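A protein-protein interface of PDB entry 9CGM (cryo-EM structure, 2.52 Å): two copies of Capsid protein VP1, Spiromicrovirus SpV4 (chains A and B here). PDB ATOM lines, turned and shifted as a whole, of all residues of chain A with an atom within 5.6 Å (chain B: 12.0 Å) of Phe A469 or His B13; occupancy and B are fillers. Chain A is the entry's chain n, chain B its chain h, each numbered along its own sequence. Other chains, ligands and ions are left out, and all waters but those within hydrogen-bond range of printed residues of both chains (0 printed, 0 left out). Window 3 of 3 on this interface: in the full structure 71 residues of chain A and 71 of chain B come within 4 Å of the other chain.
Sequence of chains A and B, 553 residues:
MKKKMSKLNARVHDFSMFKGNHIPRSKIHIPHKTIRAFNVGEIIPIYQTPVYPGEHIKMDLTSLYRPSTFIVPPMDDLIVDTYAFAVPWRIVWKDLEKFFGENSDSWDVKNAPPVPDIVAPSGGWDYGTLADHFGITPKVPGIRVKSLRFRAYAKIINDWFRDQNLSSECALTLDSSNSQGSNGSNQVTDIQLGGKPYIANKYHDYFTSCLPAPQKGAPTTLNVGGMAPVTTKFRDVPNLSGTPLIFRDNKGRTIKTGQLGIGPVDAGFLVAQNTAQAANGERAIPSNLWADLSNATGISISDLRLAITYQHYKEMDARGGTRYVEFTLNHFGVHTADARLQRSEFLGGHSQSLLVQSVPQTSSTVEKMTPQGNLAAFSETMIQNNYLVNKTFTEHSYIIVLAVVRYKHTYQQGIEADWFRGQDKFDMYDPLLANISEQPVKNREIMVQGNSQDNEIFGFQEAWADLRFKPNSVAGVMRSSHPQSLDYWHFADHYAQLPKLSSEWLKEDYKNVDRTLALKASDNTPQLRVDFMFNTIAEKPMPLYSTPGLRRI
The backbone carbonyl oxygen (O) of Tyr A206 lies close to the side-chain amide oxygen (OE1) of Gln A461.
His A204 touches Phe B15. Asp A205 touches Phe B15 (O to CE2, 3.2 Å). CZ of Phe B15 touches NE2 of Gln A461, at 3.96 Å. His B13 touches Phe A469 (ND1 to CE1, 3.1 Å). Phe A469 touches Phe B15 (CZ to CZ, 3.2 Å).
Of the printed residues of chain B, Phe A469 touches His B13 and Phe B15. Of chain A, only Phe A469 comes within 4 Å of His B13. No residue of chain B comes within 4 Å of Ala A465. No residue of chain B comes within 4 Å of Asp A466. No residue of chain B comes within 4 Å of Lys A470. No residue of chain B comes within 4 Å of Pro A471. Of the printed residues of chain B, His A204 touches Phe B15 (3.6 Å). Of the printed residues of chain A, Phe B15 touches His A204, Asp A205, Gln A461 and Phe A469. Of the printed residues of chain B, Gln A461 touches Phe B15. Arg A468 touches none of the printed residues of chain B. Val B12 touches none of the printed residues of chain A.
Printed residues of chain A that touch a printed residue of chain B: His A204, Asp A205, Gln A461 and Phe A469. Hydrophobic or aromatic side chains of chain A that line the printed part of chain B: His A204 and Phe A469. Of the 9 printed residues of chain B, 2 touch a printed residue of chain A. Hydrophobic or aromatic side chains of chain B that line the printed part of chain A: His B13 and Phe B15. Among the printed residues, no Asp or Glu carboxylate lies within 4 Å of a Lys or Arg side-chain nitrogen of the other chain.
No position is printed for both chains.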
ATOM      1  N   HIS A 204     -31.083  10.176 -24.029  1.00  0.00           N
ATOM      2  CA  HIS A 204     -30.223  11.341 -24.174  1.00  0.00           C
ATOM      3  C   HIS A 204     -28.770  10.927 -24.354  1.00  0.00           C
ATOM      4  O   HIS A 204     -28.215  10.198 -23.531  1.00  0.00           O
ATOM      5  CB  HIS A 204     -30.357  12.239 -22.948  1.00  0.00           C
ATOM      6  CG  HIS A 204     -31.709  12.854 -22.786  1.00  0.00           C
ATOM      7  ND1 HIS A 204     -32.113  13.955 -23.503  1.00  0.00           N
ATOM      8  CD2 HIS A 204     -32.763  12.499 -22.015  1.00  0.00           C
ATOM      9  CE1 HIS A 204     -33.348  14.270 -23.161  1.00  0.00           C
ATOM     10  NE2 HIS A 204     -33.768  13.398 -22.267  1.00  0.00           N
ATOM     11  N   ASP A 205     -28.153  11.406 -25.425  1.00  0.00           N
ATOM     12  CA  ASP A 205     -26.718  11.279 -25.612  1.00  0.00           C
ATOM     13  C   ASP A 205     -26.267  12.504 -26.393  1.00  0.00           C
ATOM     14  O   ASP A 205     -27.019  13.471 -26.530  1.00  0.00           O
ATOM     15  CB  ASP A 205     -26.350   9.934 -26.271  1.00  0.00           C
ATOM     16  CG  ASP A 205     -26.792   9.820 -27.722  1.00  0.00           C
ATOM     17  OD1 ASP A 205     -27.160  10.821 -28.355  1.00  0.00           O
ATOM     18  OD2 ASP A 205     -26.770   8.696 -28.245  1.00  0.00           O
ATOM     19  N   TYR A 206     -25.036  12.468 -26.898  1.00  0.00           N
ATOM     20  CA  TYR A 206     -24.490  13.607 -27.626  1.00  0.00           C
ATOM     21  C   TYR A 206     -25.387  14.029 -28.780  1.00  0.00           C
ATOM     22  O   TYR A 206     -25.699  15.213 -28.925  1.00  0.00           O
ATOM     23  CB  TYR A 206     -23.091  13.267 -28.127  1.00  0.00           C
ATOM     24  CG  TYR A 206     -22.418  14.354 -28.929  1.00  0.00           C
ATOM     25  CD1 TYR A 206     -21.912  15.484 -28.308  1.00  0.00           C
ATOM     26  CD2 TYR A 206     -22.244  14.228 -30.296  1.00  0.00           C
ATOM     27  CE1 TYR A 206     -21.286  16.465 -29.029  1.00  0.00           C
ATOM     28  CE2 TYR A 206     -21.617  15.205 -31.021  1.00  0.00           C
ATOM     29  CZ  TYR A 206     -21.137  16.320 -30.384  1.00  0.00           C
ATOM     30  OH  TYR A 206     -20.505  17.300 -31.102  1.00  0.00           O
ATOM     31  N   GLN A 461     -25.339  22.015 -30.043  1.00  0.00           N
ATOM     32  CA  GLN A 461     -24.986  21.457 -28.756  1.00  0.00           C
ATOM     33  C   GLN A 461     -24.310  22.566 -27.968  1.00  0.00           C
ATOM     34  O   GLN A 461     -23.959  23.603 -28.526  1.00  0.00           O
ATOM     35  CB  GLN A 461     -24.086  20.235 -28.953  1.00  0.00           C
ATOM     36  CG  GLN A 461     -23.835  19.408 -27.739  1.00  0.00           C
ATOM     37  CD  GLN A 461     -25.049  18.692 -27.252  1.00  0.00           C
ATOM     38  OE1 GLN A 461     -25.624  17.887 -27.961  1.00  0.00           O
ATOM     39  NE2 GLN A 461     -25.442  18.970 -26.030  1.00  0.00           N
ATOM     40  N   GLU A 462     -24.140  22.370 -26.665  1.00  0.00           N
ATOM     41  CA  GLU A 462     -23.425  23.378 -25.897  1.00  0.00           C
ATOM     42  C   GLU A 462     -21.995  23.474 -26.407  1.00  0.00           C
ATOM     43  O   GLU A 462     -21.471  22.534 -27.009  1.00  0.00           O
ATOM     44  CB  GLU A 462     -23.407  23.061 -24.406  1.00  0.00           C
ATOM     45  CG  GLU A 462     -22.522  21.898 -24.063  1.00  0.00           C
ATOM     46  CD  GLU A 462     -22.335  21.688 -22.571  1.00  0.00           C
ATOM     47  OE1 GLU A 462     -22.609  22.622 -21.792  1.00  0.00           O
ATOM     48  OE2 GLU A 462     -21.884  20.592 -22.178  1.00  0.00           O
ATOM     49  N   ALA A 465     -18.831  20.618 -26.281  1.00  0.00           N
ATOM     50  CA  ALA A 465     -19.417  19.437 -25.663  1.00  0.00           C
ATOM     51  C   ALA A 465     -18.740  18.156 -26.121  1.00  0.00           C
ATOM     52  O   ALA A 465     -18.765  17.156 -25.399  1.00  0.00           O
ATOM     53  CB  ALA A 465     -20.908  19.371 -25.960  1.00  0.00           C
ATOM     54  N   ASP A 466     -18.139  18.155 -27.307  1.00  0.00           N
ATOM     55  CA  ASP A 466     -17.439  16.965 -27.762  1.00  0.00           C
ATOM     56  C   ASP A 466     -16.236  16.646 -26.892  1.00  0.00           C
ATOM     57  O   ASP A 466     -15.740  15.518 -26.924  1.00  0.00           O
ATOM     58  CB  ASP A 466     -17.000  17.133 -29.207  1.00  0.00           C
ATOM     59  CG  ASP A 466     -16.086  18.308 -29.393  1.00  0.00           C
ATOM     60  OD1 ASP A 466     -15.943  19.099 -28.443  1.00  0.00           O
ATOM     61  OD2 ASP A 466     -15.487  18.432 -30.474  1.00  0.00           O
ATOM     62  N   LEU A 467     -15.742  17.615 -26.133  1.00  0.00           N
ATOM     63  CA  LEU A 467     -14.716  17.334 -25.147  1.00  0.00           C
ATOM     64  C   LEU A 467     -15.279  16.752 -23.865  1.00  0.00           C
ATOM     65  O   LEU A 467     -14.507  16.306 -23.017  1.00  0.00           O
ATOM     66  CB  LEU A 467     -13.929  18.598 -24.838  1.00  0.00           C
ATOM     67  CG  LEU A 467     -13.088  19.091 -26.005  1.00  0.00           C
ATOM     68  CD1 LEU A 467     -12.435  20.402 -25.659  1.00  0.00           C
ATOM     69  CD2 LEU A 467     -12.050  18.054 -26.343  1.00  0.00           C
ATOM     70  N   ARG A 468     -16.595  16.783 -23.686  1.00  0.00           N
ATOM     71  CA  ARG A 468     -17.241  16.114 -22.574  1.00  0.00           C
ATOM     72  C   ARG A 468     -17.873  14.781 -22.944  1.00  0.00           C
ATOM     73  O   ARG A 468     -18.375  14.090 -22.056  1.00  0.00           O
ATOM     74  CB  ARG A 468     -18.305  17.037 -21.966  1.00  0.00           C
ATOM     75  CG  ARG A 468     -17.747  18.309 -21.382  1.00  0.00           C
ATOM     76  CD  ARG A 468     -18.844  19.129 -20.789  1.00  0.00           C
ATOM     77  NE  ARG A 468     -18.368  20.356 -20.168  1.00  0.00           N
ATOM     78  CZ  ARG A 468     -18.206  21.506 -20.808  1.00  0.00           C
ATOM     79  NH1 ARG A 468     -18.490  21.593 -22.096  1.00  0.00           N
ATOM     80  NH2 ARG A 468     -17.777  22.572 -20.151  1.00  0.00           N
ATOM     81  N   PHE A 469     -17.858  14.402 -24.214  1.00  0.00           N
ATOM     82  CA  PHE A 469     -18.552  13.222 -24.705  1.00  0.00           C
ATOM     83  C   PHE A 469     -17.670  12.473 -25.683  1.00  0.00           C
ATOM     84  O   PHE A 469     -16.918  13.083 -26.443  1.00  0.00           O
ATOM     85  CB  PHE A 469     -19.849  13.584 -25.422  1.00  0.00           C
ATOM     86  CG  PHE A 469     -20.913  14.111 -24.531  1.00  0.00           C
ATOM     87  CD1 PHE A 469     -21.829  13.264 -23.957  1.00  0.00           C
ATOM     88  CD2 PHE A 469     -20.995  15.459 -24.261  1.00  0.00           C
ATOM     89  CE1 PHE A 469     -22.814  13.757 -23.151  1.00  0.00           C
ATOM     90  CE2 PHE A 469     -21.967  15.953 -23.444  1.00  0.00           C
ATOM     91  CZ  PHE A 469     -22.878  15.102 -22.890  1.00  0.00           C
ATOM     92  N   LYS A 470     -17.771  11.151 -25.673  1.00  0.00           N
ATOM     93  CA  LYS A 470     -17.136  10.329 -26.698  1.00  0.00           C
ATOM     94  C   LYS A 470     -18.139   9.282 -27.156  1.00  0.00           C
ATOM     95  O   LYS A 470     -18.241   8.207 -26.543  1.00  0.00           O
ATOM     96  CB  LYS A 470     -15.844   9.704 -26.197  1.00  0.00           C
ATOM     97  CG  LYS A 470     -15.043   9.120 -27.319  1.00  0.00           C
ATOM     98  CD  LYS A 470     -13.654   8.748 -26.909  1.00  0.00           C
ATOM     99  CE  LYS A 470     -12.895   8.280 -28.124  1.00  0.00           C
ATOM    100  NZ  LYS A 470     -11.482   8.012 -27.840  1.00  0.00           N
ATOM    101  N   PRO A 471     -18.915   9.571 -28.201  1.00  0.00           N
ATOM    102  CA  PRO A 471     -19.967   8.645 -28.635  1.00  0.00           C
ATOM    103  C   PRO A 471     -19.449   7.236 -28.876  1.00  0.00           C
ATOM    104  O   PRO A 471     -18.329   7.036 -29.348  1.00  0.00           O
ATOM    105  CB  PRO A 471     -20.466   9.276 -29.938  1.00  0.00           C
ATOM    106  CG  PRO A 471     -20.148  10.710 -29.796  1.00  0.00           C
ATOM    107  CD  PRO A 471     -18.886  10.794 -29.016  1.00  0.00           C
ATOM    108  N   ALA B  10     -21.561   0.642 -14.454  1.00  0.00           N
ATOM    109  CA  ALA B  10     -22.809   0.798 -13.722  1.00  0.00           C
ATOM    110  C   ALA B  10     -23.366   2.211 -13.892  1.00  0.00           C
ATOM    111  O   ALA B  10     -24.570   2.437 -13.748  1.00  0.00           O
ATOM    112  CB  ALA B  10     -22.601   0.477 -12.254  1.00  0.00           C
ATOM    113  N   ARG B  11     -22.483   3.157 -14.208  1.00  0.00           N
ATOM    114  CA  ARG B  11     -22.864   4.547 -14.408  1.00  0.00           C
ATOM    115  C   ARG B  11     -22.463   4.993 -15.806  1.00  0.00           C
ATOM    116  O   ARG B  11     -21.367   4.681 -16.280  1.00  0.00           O
ATOM    117  CB  ARG B  11     -22.214   5.457 -13.362  1.00  0.00           C
ATOM    118  CG  ARG B  11     -20.695   5.494 -13.409  1.00  0.00           C
ATOM    119  CD  ARG B  11     -20.161   6.407 -12.340  1.00  0.00           C
ATOM    120  NE  ARG B  11     -20.651   7.770 -12.511  1.00  0.00           N
ATOM    121  CZ  ARG B  11     -20.426   8.753 -11.648  1.00  0.00           C
ATOM    122  NH1 ARG B  11     -19.714   8.527 -10.552  1.00  0.00           N
ATOM    123  NH2 ARG B  11     -20.914   9.963 -11.880  1.00  0.00           N
ATOM    124  N   VAL B  12     -23.369   5.709 -16.473  1.00  0.00           N
ATOM    125  CA  VAL B  12     -23.131   6.260 -17.801  1.00  0.00           C
ATOM    126  C   VAL B  12     -23.671   7.687 -17.781  1.00  0.00           C
ATOM    127  O   VAL B  12     -24.272   8.127 -16.799  1.00  0.00           O
ATOM    128  CB  VAL B  12     -23.788   5.376 -18.898  1.00  0.00           C
ATOM    129  CG1 VAL B  12     -23.671   5.948 -20.301  1.00  0.00           C
ATOM    130  CG2 VAL B  12     -23.151   3.991 -18.888  1.00  0.00           C
ATOM    131  N   HIS B  13     -23.449   8.416 -18.873  1.00  0.00           N
ATOM    132  CA  HIS B  13     -23.745   9.843 -18.907  1.00  0.00           C
ATOM    133  C   HIS B  13     -25.147  10.021 -19.470  1.00  0.00           C
ATOM    134  O   HIS B  13     -25.411   9.790 -20.653  1.00  0.00           O
ATOM    135  CB  HIS B  13     -22.688  10.582 -19.721  1.00  0.00           C
ATOM    136  CG  HIS B  13     -22.758  12.072 -19.598  1.00  0.00           C
ATOM    137  ND1 HIS B  13     -21.954  12.918 -20.331  1.00  0.00           N
ATOM    138  CD2 HIS B  13     -23.540  12.867 -18.831  1.00  0.00           C
ATOM    139  CE1 HIS B  13     -22.227  14.170 -20.005  1.00  0.00           C
ATOM    140  NE2 HIS B  13     -23.192  14.166 -19.105  1.00  0.00           N
ATOM    141  N   ASP B  14     -26.062  10.428 -18.592  1.00  0.00           N
ATOM    142  CA  ASP B  14     -27.430  10.778 -18.944  1.00  0.00           C
ATOM    143  C   ASP B  14     -27.616  12.252 -18.626  1.00  0.00           C
ATOM    144  O   ASP B  14     -27.298  12.686 -17.513  1.00  0.00           O
ATOM    145  CB  ASP B  14     -28.440   9.942 -18.154  1.00  0.00           C
ATOM    146  CG  ASP B  14     -28.355   8.453 -18.474  1.00  0.00           C
ATOM    147  OD1 ASP B  14     -27.704   8.086 -19.477  1.00  0.00           O
ATOM    148  OD2 ASP B  14     -28.953   7.650 -17.724  1.00  0.00           O
ATOM    149  N   PHE B  15     -28.113  13.017 -19.592  1.00  0.00           N
ATOM    150  CA  PHE B  15     -28.219  14.458 -19.408  1.00  0.00           C
ATOM    151  C   PHE B  15     -29.051  14.815 -18.191  1.00  0.00           C
ATOM    152  O   PHE B  15     -29.954  14.076 -17.793  1.00  0.00           O
ATOM    153  CB  PHE B  15     -28.808  15.118 -20.648  1.00  0.00           C
ATOM    154  CG  PHE B  15     -27.809  15.370 -21.718  1.00  0.00           C
ATOM    155  CD1 PHE B  15     -27.163  16.591 -21.797  1.00  0.00           C
ATOM    156  CD2 PHE B  15     -27.462  14.373 -22.602  1.00  0.00           C
ATOM    157  CE1 PHE B  15     -26.240  16.832 -22.774  1.00  0.00           C
ATOM    158  CE2 PHE B  15     -26.530  14.603 -23.566  1.00  0.00           C
ATOM    159  CZ  PHE B  15     -25.927  15.836 -23.664  1.00  0.00           C
ATOM    160  N   SER B  16     -28.723  15.958 -17.595  1.00  0.00           N
ATOM    161  CA  SER B  16     -29.404  16.427 -16.400  1.00  0.00           C
ATOM    162  C   SER B  16     -29.490  17.945 -16.410  1.00  0.00           C
ATOM    163  O   SER B  16     -28.991  18.601 -17.329  1.00  0.00           O
ATOM    164  CB  SER B  16     -28.676  15.937 -15.150  1.00  0.00           C
ATOM    165  OG  SER B  16     -27.366  16.467 -15.090  1.00  0.00           O
ATOM    166  N   MET B  17     -30.107  18.502 -15.377  1.00  0.00           N
ATOM    167  CA  MET B  17     -30.378  19.927 -15.314  1.00  0.00           C
ATOM    168  C   MET B  17     -29.104  20.710 -15.016  1.00  0.00           C
ATOM    169  O   MET B  17     -28.255  20.290 -14.224  1.00  0.00           O
ATOM    170  CB  MET B  17     -31.435  20.206 -14.243  1.00  0.00           C
ATOM    171  CG  MET B  17     -31.784  21.667 -14.050  1.00  0.00           C
ATOM    172  SD  MET B  17     -33.066  21.895 -12.806  1.00  0.00           S
ATOM    173  CE  MET B  17     -32.180  21.497 -11.301  1.00  0.00           C
ATOM    174  N   PHE B  18     -28.983  21.866 -15.661  1.00  0.00           N
ATOM    175  CA  PHE B  18     -27.889  22.797 -15.434  1.00  0.00           C
ATOM    176  C   PHE B  18     -27.998  23.485 -14.079  1.00  0.00           C
ATOM    177  O   PHE B  18     -27.109  24.262 -13.715  1.00  0.00           O
ATOM    178  CB  PHE B  18     -27.874  23.854 -16.538  1.00  0.00           C
ATOM    179  CG  PHE B  18     -27.708  23.298 -17.922  1.00  0.00           C
ATOM    180  CD1 PHE B  18     -26.460  23.184 -18.492  1.00  0.00           C
ATOM    181  CD2 PHE B  18     -28.812  22.877 -18.653  1.00  0.00           C
ATOM    182  CE1 PHE B  18     -26.312  22.684 -19.774  1.00  0.00           C
ATOM    183  CE2 PHE B  18     -28.670  22.366 -19.931  1.00  0.00           C
ATOM    184  CZ  PHE B  18     -27.421  22.268 -20.493  1.00  0.00           C
